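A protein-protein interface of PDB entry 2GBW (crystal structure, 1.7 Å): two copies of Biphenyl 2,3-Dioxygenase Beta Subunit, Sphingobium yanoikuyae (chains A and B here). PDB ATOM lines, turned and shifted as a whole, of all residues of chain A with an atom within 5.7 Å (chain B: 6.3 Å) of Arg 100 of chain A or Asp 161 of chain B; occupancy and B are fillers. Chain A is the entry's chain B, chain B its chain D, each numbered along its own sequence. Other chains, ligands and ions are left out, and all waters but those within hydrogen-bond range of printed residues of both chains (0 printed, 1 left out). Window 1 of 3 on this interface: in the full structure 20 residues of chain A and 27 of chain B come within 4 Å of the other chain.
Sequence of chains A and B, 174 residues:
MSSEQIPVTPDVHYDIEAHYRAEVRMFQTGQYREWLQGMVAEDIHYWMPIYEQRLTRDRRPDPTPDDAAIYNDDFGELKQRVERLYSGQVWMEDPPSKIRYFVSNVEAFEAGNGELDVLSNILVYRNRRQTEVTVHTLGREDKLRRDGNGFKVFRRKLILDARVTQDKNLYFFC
The side-chain amide nitrogen of Asn 121 of chain B is in hydrogen-bond range of the side-chain amide oxygen of Gln 28 of chain A (2.8 Å). O of Leu 160 of chain B sits at hydrogen-bond distance from NZ of Lys 98 of chain A (3.0 Å). NH1 of Arg 100 of chain A lies within hydrogen-bond range of OD1 of Asn 121 of chain B, 2.9 Å away. The guanidinium group of Arg 100 of chain A sits close to the backbone carbonyl oxygen of Leu 138 of chain B. The guanidinium group of Arg 100 of chain A lies within salt-bridge range of the side-chain carboxylate of Asp 161 of chain B, at 2.7 Å. O of Tyr 101 of chain A is in hydrogen-bond range of ND2 of Asn 121 of chain B (2.9 Å). N of Gly 139 of chain B sits close to NH2 of Arg 100 of chain A, 3.4 Å away.
The backbone NH (N) of Tyr 101 of chain A is in hydrogen-bond range of the side-chain amide oxygen (OE1) of Gln 28 of chain A (2.9 Å). The backbone NH (N) of Lys 98 of chain A is in hydrogen-bond range of the backbone carbonyl oxygen (O) of Asn 127 of chain A (2.9 Å). The backbone carbonyl oxygen of Tyr 125 of chain A lies within hydrogen-bond range of the backbone NH of Arg 100 of chain A, 2.8 Å away. The backbone carbonyl oxygen of Leu 123 of chain A sits at hydrogen-bond distance from the backbone NH of Phe 102 of chain A, at 2.8 Å. O of Leu 138 of chain B lies within hydrogen-bond range of N of Ile 122 of chain B (2.9 Å). The backbone NH of Ile 159 of chain B lies within hydrogen-bond range of the backbone carbonyl oxygen of Gly 139 of chain B (2.7 Å).
Lys 98 of chain A touches Ile 159 of chain B (NZ to CG2, 3.9 Å). CD of Lys 98 of chain A touches O of Asp 161 of chain B, 3.5 Å away. CB of Asn 121 of chain B touches CE2 of Phe 102 of chain A, at 3.7 Å. CZ of Phe 102 of chain A touches C of Ile 122 of chain B, 3.6 Å away. N of Leu 123 of chain B touches CE2 of Phe 102 of chain A (3.5 Å). CD2 of Leu 123 of chain A touches CD2 of Leu 123 of chain B, 3.5 Å away. Tyr 125 of chain A touches Thr 137 of chain B (CG to CG2, 3.6 Å). Asp 161 of chain B touches Asn 127 of chain A (O to CB, 3.4 Å). CB of Ala 162 of chain B touches ND2 of Asn 127 of chain A (3.7 Å).
Of the printed residues of chain B, Arg 100 of chain A touches Asn 121, Leu 138, Gly 139 and Asp 161. Of the printed residues of chain A, Asp 161 of chain B touches Lys 98 (3.5 Å), Arg 100 (2.7 Å) and Asn 127 (3.4 Å). Of the printed residues of chain A, Asn 121 of chain B touches Gln 28 (2.8 Å), Arg 100 (2.9 Å), Tyr 101 (2.9 Å) and Phe 102 (3.7 Å). Of the printed residues of chain A, Leu 123 of chain B touches Phe 102 (3.5 Å) and Leu 123 (3.5 Å). Of the printed residues of chain A, Thr 137 of chain B touches Tyr 125 (3.6 Å). Printed residues of chain A within 4 Å of Ile 159 of chain B: Lys 98 (3.9 Å). Arg 126 of chain A touches none of the printed residues of chain B. Gln 53 of chain B touches none of the printed residues of chain A. The nearest residue of chain B that does not touch Arg 100 of chain A is Ile 159 of chain B (4.2 Å). The nearest printed residue of chain A that does not touch Leu 123 of chain B is Tyr 125 of chain A (4.02 Å).
Printed residues of chain A that touch a printed residue of chain B: Gln 28, Lys 98, Arg 100, Tyr 101, Phe 102, Leu 123, Tyr 125 and Asn 127. Hydrophobic or aromatic side chains of chain A within 4 Å of the printed part of chain B: Phe 102, Leu 123 and Tyr 125. Of the 14 printed residues of chain B, 10 touch a printed residue of chain A. Printed residues of chain B that touch a printed residue of chain A: Asn 121, Ile 122, Leu 123, Thr 137, Leu 138, Gly 139, Ile 159, Leu 160, Asp 161 and Ala 162. Hydrophobic or aromatic side chains of chain B within 4 Å of the printed part of chain A: Leu 123, Ile 159 and Ala 162. Along chain B the printed residues that touch a printed residue of chain A span positions 121 to 162. Among the printed residues, Asp or Glu carboxylates within 4 Å of a Lys or Arg side-chain nitrogen of the other chain: Arg 100 of chain A with Asp 161 of chain B (2.7 Å).
Leu 123 of chain B touches its own counterpart, Leu 123 of chain A.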
ATOM      1  N   GLN A  28     -22.577  26.491 -24.016  1.00  0.00           N
ATOM      2  CA  GLN A  28     -22.296  25.165 -23.472  1.00  0.00           C
ATOM      3  C   GLN A  28     -20.845  25.011 -23.049  1.00  0.00           C
ATOM      4  O   GLN A  28     -20.543  24.184 -22.163  1.00  0.00           O
ATOM      5  CB  GLN A  28     -22.684  24.025 -24.437  1.00  0.00           C
ATOM      6  CG  GLN A  28     -24.173  23.900 -24.622  1.00  0.00           C
ATOM      7  CD  GLN A  28     -24.663  22.858 -25.633  1.00  0.00           C
ATOM      8  OE1 GLN A  28     -25.877  22.756 -25.881  1.00  0.00           O
ATOM      9  NE2 GLN A  28     -23.750  22.090 -26.200  1.00  0.00           N
ATOM     10  N   LYS A  98     -23.697  21.953 -15.758  1.00  0.00           N
ATOM     11  CA  LYS A  98     -23.802  21.561 -17.142  1.00  0.00           C
ATOM     12  C   LYS A  98     -25.087  22.106 -17.745  1.00  0.00           C
ATOM     13  O   LYS A  98     -26.113  22.178 -17.054  1.00  0.00           O
ATOM     14  CB  LYS A  98     -23.812  20.046 -17.205  1.00  0.00           C
ATOM     15  CG  LYS A  98     -22.475  19.440 -16.848  1.00  0.00           C
ATOM     16  CD  LYS A  98     -22.297  18.094 -17.537  1.00  0.00           C
ATOM     17  CE  LYS A  98     -20.802  17.602 -17.575  1.00  0.00           C
ATOM     18  NZ  LYS A  98     -20.637  16.180 -18.147  1.00  0.00           N
ATOM     19  N   ILE A  99     -25.041  22.512 -19.005  1.00  0.00           N
ATOM     20  CA  ILE A  99     -26.263  23.005 -19.631  1.00  0.00           C
ATOM     21  C   ILE A  99     -26.237  22.531 -21.084  1.00  0.00           C
ATOM     22  O   ILE A  99     -25.154  22.431 -21.697  1.00  0.00           O
ATOM     23  CB  ILE A  99     -26.378  24.522 -19.501  1.00  0.00           C
ATOM     24  CG1 ILE A  99     -27.737  25.024 -20.028  1.00  0.00           C
ATOM     25  CG2 ILE A  99     -25.177  25.235 -20.164  1.00  0.00           C
ATOM     26  CD1 ILE A  99     -28.075  26.402 -19.538  1.00  0.00           C
ATOM     27  N   ARG A 100     -27.384  22.154 -21.593  1.00  0.00           N
ATOM     28  CA  ARG A 100     -27.479  21.728 -22.987  1.00  0.00           C
ATOM     29  C   ARG A 100     -28.733  22.253 -23.621  1.00  0.00           C
ATOM     30  O   ARG A 100     -29.788  22.150 -23.087  1.00  0.00           O
ATOM     31  CB  ARG A 100     -27.412  20.205 -23.124  1.00  0.00           C
ATOM     32  CG  ARG A 100     -27.082  19.711 -24.506  1.00  0.00           C
ATOM     33  CD  ARG A 100     -26.631  18.274 -24.657  1.00  0.00           C
ATOM     34  NE  ARG A 100     -25.509  17.916 -23.765  1.00  0.00           N
ATOM     35  CZ  ARG A 100     -24.223  18.120 -24.042  1.00  0.00           C
ATOM     36  NH1 ARG A 100     -23.807  18.630 -25.224  1.00  0.00           N
ATOM     37  NH2 ARG A 100     -23.321  17.795 -23.137  1.00  0.00           N
ATOM     38  N   TYR A 101     -28.600  22.790 -24.826  1.00  0.00           N
ATOM     39  CA  TYR A 101     -29.704  23.511 -25.482  1.00  0.00           C
ATOM     40  C   TYR A 101     -30.154  22.812 -26.769  1.00  0.00           C
ATOM     41  O   TYR A 101     -29.341  22.394 -27.609  1.00  0.00           O
ATOM     42  CB  TYR A 101     -29.252  24.929 -25.922  1.00  0.00           C
ATOM     43  CG  TYR A 101     -28.820  25.907 -24.871  1.00  0.00           C
ATOM     44  CD1 TYR A 101     -27.562  25.830 -24.289  1.00  0.00           C
ATOM     45  CD2 TYR A 101     -29.604  26.993 -24.544  1.00  0.00           C
ATOM     46  CE1 TYR A 101     -27.142  26.743 -23.331  1.00  0.00           C
ATOM     47  CE2 TYR A 101     -29.189  27.905 -23.573  1.00  0.00           C
ATOM     48  CZ  TYR A 101     -27.964  27.787 -22.991  1.00  0.00           C
ATOM     49  OH  TYR A 101     -27.540  28.730 -22.086  1.00  0.00           O
ATOM     50  N   PHE A 102     -31.471  22.716 -26.917  1.00  0.00           N
ATOM     51  CA  PHE A 102     -32.111  22.144 -28.069  1.00  0.00           C
ATOM     52  C   PHE A 102     -32.981  23.202 -28.729  1.00  0.00           C
ATOM     53  O   PHE A 102     -34.039  23.554 -28.226  1.00  0.00           O
ATOM     54  CB  PHE A 102     -32.882  20.899 -27.673  1.00  0.00           C
ATOM     55  CG  PHE A 102     -31.995  19.796 -27.139  1.00  0.00           C
ATOM     56  CD1 PHE A 102     -31.606  19.821 -25.836  1.00  0.00           C
ATOM     57  CD2 PHE A 102     -31.571  18.725 -27.965  1.00  0.00           C
ATOM     58  CE1 PHE A 102     -30.752  18.837 -25.306  1.00  0.00           C
ATOM     59  CE2 PHE A 102     -30.687  17.719 -27.452  1.00  0.00           C
ATOM     60  CZ  PHE A 102     -30.328  17.759 -26.101  1.00  0.00           C
ATOM     61  N   LEU A 123     -35.376  24.443 -25.809  1.00  0.00           N
ATOM     62  CA  LEU A 123     -35.447  23.521 -24.684  1.00  0.00           C
ATOM     63  C   LEU A 123     -34.061  23.474 -24.040  1.00  0.00           C
ATOM     64  O   LEU A 123     -33.060  23.189 -24.694  1.00  0.00           O
ATOM     65  CB  LEU A 123     -35.829  22.106 -25.187  1.00  0.00           C
ATOM     66  CG  LEU A 123     -35.856  20.932 -24.195  1.00  0.00           C
ATOM     67  CD1 LEU A 123     -36.816  21.133 -23.028  1.00  0.00           C
ATOM     68  CD2 LEU A 123     -36.192  19.627 -24.983  1.00  0.00           C
ATOM     69  N   VAL A 124     -34.031  23.715 -22.738  1.00  0.00           N
ATOM     70  CA  VAL A 124     -32.771  23.850 -21.984  1.00  0.00           C
ATOM     71  C   VAL A 124     -32.776  22.834 -20.881  1.00  0.00           C
ATOM     72  O   VAL A 124     -33.685  22.829 -20.052  1.00  0.00           O
ATOM     73  CB  VAL A 124     -32.583  25.248 -21.309  1.00  0.00           C
ATOM     74  CG1 VAL A 124     -31.225  25.272 -20.562  1.00  0.00           C
ATOM     75  CG2 VAL A 124     -32.670  26.380 -22.351  1.00  0.00           C
ATOM     76  N   TYR A 125     -31.821  21.923 -20.946  1.00  0.00           N
ATOM     77  CA  TYR A 125     -31.610  20.907 -19.951  1.00  0.00           C
ATOM     78  C   TYR A 125     -30.359  21.248 -19.140  1.00  0.00           C
ATOM     79  O   TYR A 125     -29.283  21.384 -19.678  1.00  0.00           O
ATOM     80  CB  TYR A 125     -31.390  19.524 -20.599  1.00  0.00           C
ATOM     81  CG  TYR A 125     -32.493  18.569 -20.421  1.00  0.00           C
ATOM     82  CD1 TYR A 125     -33.581  18.589 -21.272  1.00  0.00           C
ATOM     83  CD2 TYR A 125     -32.458  17.640 -19.413  1.00  0.00           C
ATOM     84  CE1 TYR A 125     -34.632  17.719 -21.092  1.00  0.00           C
ATOM     85  CE2 TYR A 125     -33.476  16.755 -19.251  1.00  0.00           C
ATOM     86  CZ  TYR A 125     -34.567  16.817 -20.097  1.00  0.00           C
ATOM     87  OH  TYR A 125     -35.622  15.961 -19.908  1.00  0.00           O
ATOM     88  N   ARG A 126     -30.520  21.262 -17.822  1.00  0.00           N
ATOM     89  CA  ARG A 126     -29.454  21.592 -16.888  1.00  0.00           C
ATOM     90  C   ARG A 126     -29.236  20.475 -15.879  1.00  0.00           C
ATOM     91  O   ARG A 126     -30.208  19.908 -15.350  1.00  0.00           O
ATOM     92  CB  ARG A 126     -29.772  22.880 -16.120  1.00  0.00           C
ATOM     93  CG  ARG A 126     -30.165  24.101 -16.979  1.00  0.00           C
ATOM     94  CD  ARG A 126     -30.582  25.304 -16.100  1.00  0.00           C
ATOM     95  NE  ARG A 126     -29.463  26.014 -15.500  1.00  0.00           N
ATOM     96  CZ  ARG A 126     -29.553  26.972 -14.578  1.00  0.00           C
ATOM     97  NH1 ARG A 126     -30.723  27.234 -14.007  1.00  0.00           N
ATOM     98  NH2 ARG A 126     -28.469  27.602 -14.150  1.00  0.00           N
ATOM     99  N   ASN A 127     -27.967  20.167 -15.594  1.00  0.00           N
ATOM    100  CA  ASN A 127     -27.589  19.167 -14.578  1.00  0.00           C
ATOM    101  C   ASN A 127     -26.525  19.741 -13.688  1.00  0.00           C
ATOM    102  O   ASN A 127     -25.680  20.520 -14.146  1.00  0.00           O
ATOM    103  CB  ASN A 127     -26.997  17.924 -15.275  1.00  0.00           C
ATOM    104  CG  ASN A 127     -28.027  17.103 -15.971  1.00  0.00           C
ATOM    105  OD1 ASN A 127     -28.392  17.407 -17.122  1.00  0.00           O
ATOM    106  ND2 ASN A 127     -28.506  16.052 -15.309  1.00  0.00           N
ATOM    107  N   GLN B  53     -17.198  14.570 -10.553  1.00  0.00           N
ATOM    108  CA  GLN B  53     -17.299  15.954 -10.129  1.00  0.00           C
ATOM    109  C   GLN B  53     -16.050  16.316  -9.317  1.00  0.00           C
ATOM    110  O   GLN B  53     -15.782  15.696  -8.327  1.00  0.00           O
ATOM    111  CB  GLN B  53     -18.540  16.153  -9.262  1.00  0.00           C
ATOM    112  CG  GLN B  53     -19.891  15.907  -9.975  1.00  0.00           C
ATOM    113  CD  GLN B  53     -20.247  16.956 -11.006  1.00  0.00           C
ATOM    114  OE1 GLN B  53     -19.374  17.595 -11.612  1.00  0.00           O
ATOM    115  NE2 GLN B  53     -21.527  17.118 -11.254  1.00  0.00           N
ATOM    116  N   SER B 120     -22.535  17.211 -31.676  1.00  0.00           N
ATOM    117  CA  SER B 120     -23.971  17.279 -31.658  1.00  0.00           C
ATOM    118  C   SER B 120     -24.466  17.122 -30.260  1.00  0.00           C
ATOM    119  O   SER B 120     -23.725  16.585 -29.385  1.00  0.00           O
ATOM    120  CB  SER B 120     -24.618  16.241 -32.544  1.00  0.00           C
ATOM    121  OG  SER B 120     -24.220  14.919 -32.296  1.00  0.00           O
ATOM    122  N   ASN B 121     -25.680  17.605 -30.057  1.00  0.00           N
ATOM    123  CA  ASN B 121     -26.464  17.426 -28.815  1.00  0.00           C
ATOM    124  C   ASN B 121     -27.480  16.317 -28.998  1.00  0.00           C
ATOM    125  O   ASN B 121     -28.161  16.259 -30.032  1.00  0.00           O
ATOM    126  CB  ASN B 121     -27.219  18.716 -28.468  1.00  0.00           C
ATOM    127  CG  ASN B 121     -26.307  19.831 -27.949  1.00  0.00           C
ATOM    128  OD1 ASN B 121     -25.135  19.617 -27.641  1.00  0.00           O
ATOM    129  ND2 ASN B 121     -26.845  21.033 -27.857  1.00  0.00           N
ATOM    130  N   ILE B 122     -27.612  15.444 -28.011  1.00  0.00           N
ATOM    131  CA  ILE B 122     -28.579  14.396 -28.102  1.00  0.00           C
ATOM    132  C   ILE B 122     -29.459  14.326 -26.881  1.00  0.00           C
ATOM    133  O   ILE B 122     -28.949  14.344 -25.731  1.00  0.00           O
ATOM    134  CB  ILE B 122     -27.955  13.027 -28.345  1.00  0.00           C
ATOM    135  CG1 ILE B 122     -26.933  13.083 -29.476  1.00  0.00           C
ATOM    136  CG2 ILE B 122     -29.055  11.988 -28.735  1.00  0.00           C
ATOM    137  CD1 ILE B 122     -26.052  11.868 -29.599  1.00  0.00           C
ATOM    138  N   LEU B 123     -30.766  14.266 -27.140  1.00  0.00           N
ATOM    139  CA  LEU B 123     -31.780  13.984 -26.124  1.00  0.00           C
ATOM    140  C   LEU B 123     -32.410  12.618 -26.434  1.00  0.00           C
ATOM    141  O   LEU B 123     -32.864  12.337 -27.546  1.00  0.00           O
ATOM    142  CB  LEU B 123     -32.801  15.137 -26.147  1.00  0.00           C
ATOM    143  CG  LEU B 123     -34.047  15.126 -25.307  1.00  0.00           C
ATOM    144  CD1 LEU B 123     -33.667  15.029 -23.913  1.00  0.00           C
ATOM    145  CD2 LEU B 123     -34.927  16.399 -25.534  1.00  0.00           C
ATOM    146  N   THR B 137     -29.650  13.265 -21.563  1.00  0.00           N
ATOM    147  CA  THR B 137     -29.022  14.205 -22.477  1.00  0.00           C
ATOM    148  C   THR B 137     -27.520  13.986 -22.503  1.00  0.00           C
ATOM    149  O   THR B 137     -26.889  13.667 -21.483  1.00  0.00           O
ATOM    150  CB  THR B 137     -29.324  15.701 -22.191  1.00  0.00           C
ATOM    151  OG1 THR B 137     -28.900  16.086 -20.870  1.00  0.00           O
ATOM    152  CG2 THR B 137     -30.839  16.018 -22.347  1.00  0.00           C
ATOM    153  N   LEU B 138     -26.944  14.116 -23.691  1.00  0.00           N
ATOM    154  CA  LEU B 138     -25.521  13.825 -23.886  1.00  0.00           C
ATOM    155  C   LEU B 138     -24.970  14.726 -24.988  1.00  0.00           C
ATOM    156  O   LEU B 138     -25.712  15.204 -25.882  1.00  0.00           O
ATOM    157  CB  LEU B 138     -25.295  12.401 -24.422  1.00  0.00           C
ATOM    158  CG  LEU B 138     -25.871  11.132 -23.808  1.00  0.00           C
ATOM    159  CD1 LEU B 138     -27.231  10.873 -24.474  1.00  0.00           C
ATOM    160  CD2 LEU B 138     -24.900   9.914 -23.966  1.00  0.00           C
ATOM    161  N   GLY B 139     -23.685  14.974 -24.913  1.00  0.00           N
ATOM    162  CA  GLY B 139     -22.940  15.452 -26.057  1.00  0.00           C
ATOM    163  C   GLY B 139     -22.289  14.299 -26.798  1.00  0.00           C
ATOM    164  O   GLY B 139     -21.846  13.304 -26.207  1.00  0.00           O
ATOM    165  N   ARG B 140     -22.195  14.463 -28.107  1.00  0.00           N
ATOM    166  CA  ARG B 140     -21.530  13.506 -28.970  1.00  0.00           C
ATOM    167  C   ARG B 140     -20.404  14.203 -29.739  1.00  0.00           C
ATOM    168  O   ARG B 140     -20.590  15.307 -30.274  1.00  0.00           O
ATOM    169  CB  ARG B 140     -22.521  12.882 -29.925  1.00  0.00           C
ATOM    170  CG  ARG B 140     -21.867  11.881 -30.874  1.00  0.00           C
ATOM    171  CD  ARG B 140     -22.836  11.050 -31.576  1.00  0.00           C
ATOM    172  NE  ARG B 140     -23.748  11.837 -32.381  1.00  0.00           N
ATOM    173  CZ  ARG B 140     -24.754  11.343 -33.088  1.00  0.00           C
ATOM    174  NH1 ARG B 140     -25.009  10.052 -33.080  1.00  0.00           N
ATOM    175  NH2 ARG B 140     -25.488  12.161 -33.832  1.00  0.00           N
ATOM    176  N   ILE B 159     -20.642  12.111 -24.053  1.00  0.00           N
ATOM    177  CA  ILE B 159     -20.402  12.781 -22.787  1.00  0.00           C
ATOM    178  C   ILE B 159     -21.746  12.933 -22.085  1.00  0.00           C
ATOM    179  O   ILE B 159     -22.604  13.693 -22.497  1.00  0.00           O
ATOM    180  CB  ILE B 159     -19.697  14.134 -23.020  1.00  0.00           C
ATOM    181  CG1 ILE B 159     -18.263  13.927 -23.610  1.00  0.00           C
ATOM    182  CG2 ILE B 159     -19.708  14.968 -21.766  1.00  0.00           C
ATOM    183  CD1 ILE B 159     -17.737  15.160 -24.321  1.00  0.00           C
ATOM    184  N   LEU B 160     -21.969  12.159 -21.037  1.00  0.00           N
ATOM    185  CA  LEU B 160     -23.227  12.154 -20.320  1.00  0.00           C
ATOM    186  C   LEU B 160     -23.370  13.400 -19.467  1.00  0.00           C
ATOM    187  O   LEU B 160     -22.410  13.854 -18.842  1.00  0.00           O
ATOM    188  CB  LEU B 160     -23.303  10.956 -19.390  1.00  0.00           C
ATOM    189  CG  LEU B 160     -23.644   9.584 -19.908  1.00  0.00           C
ATOM    190  CD1 LEU B 160     -23.349   8.602 -18.743  1.00  0.00           C
ATOM    191  CD2 LEU B 160     -25.078   9.481 -20.374  1.00  0.00           C
ATOM    192  N   ASP B 161     -24.548  13.996 -19.415  1.00  0.00           N
ATOM    193  CA  ASP B 161     -24.695  15.208 -18.618  1.00  0.00           C
ATOM    194  C   ASP B 161     -24.925  14.931 -17.122  1.00  0.00           C
ATOM    195  O   ASP B 161     -24.583  15.787 -16.353  1.00  0.00           O
ATOM    196  CB  ASP B 161     -25.848  16.065 -19.150  1.00  0.00           C
ATOM    197  CG  ASP B 161     -25.522  16.736 -20.454  1.00  0.00           C
ATOM    198  OD1 ASP B 161     -24.326  16.833 -20.779  1.00  0.00           O
ATOM    199  OD2 ASP B 161     -26.463  17.170 -21.144  1.00  0.00           O
ATOM    200  N   ALA B 162     -25.510  13.781 -16.780  1.00  0.00           N
ATOM    201  CA  ALA B 162     -25.816  13.421 -15.387  1.00  0.00           C
ATOM    202  C   ALA B 162     -24.695  12.606 -14.746  1.00  0.00           C
ATOM    203  O   ALA B 162     -24.308  11.576 -15.301  1.00  0.00           O
ATOM    204  CB  ALA B 162     -27.125  12.643 -15.297  1.00  0.00           C
ATOM    205  N   ARG B 163     -24.247  13.003 -13.564  1.00  0.00           N
ATOM    206  CA  ARG B 163     -23.304  12.199 -12.790  1.00  0.00           C
ATOM    207  C   ARG B 163     -23.918  10.871 -12.355  1.00  0.00           C
ATOM    208  O   ARG B 163     -23.281   9.859 -12.471  1.00  0.00           O
ATOM    209  CB  ARG B 163     -22.787  12.967 -11.551  1.00  0.00           C
ATOM    210  CG  ARG B 163     -21.807  12.184 -10.718  1.00  0.00           C
ATOM    211  CD  ARG B 163     -20.547  11.755 -11.507  1.00  0.00           C
ATOM    212  NE  ARG B 163     -19.628  10.913 -10.706  1.00  0.00           N
ATOM    213  CZ  ARG B 163     -19.470   9.597 -10.849  1.00  0.00           C
ATOM    214  NH1 ARG B 163     -20.291   8.894 -11.624  1.00  0.00           N
ATOM    215  NH2 ARG B 163     -18.531   8.981 -10.146  1.00  0.00           N
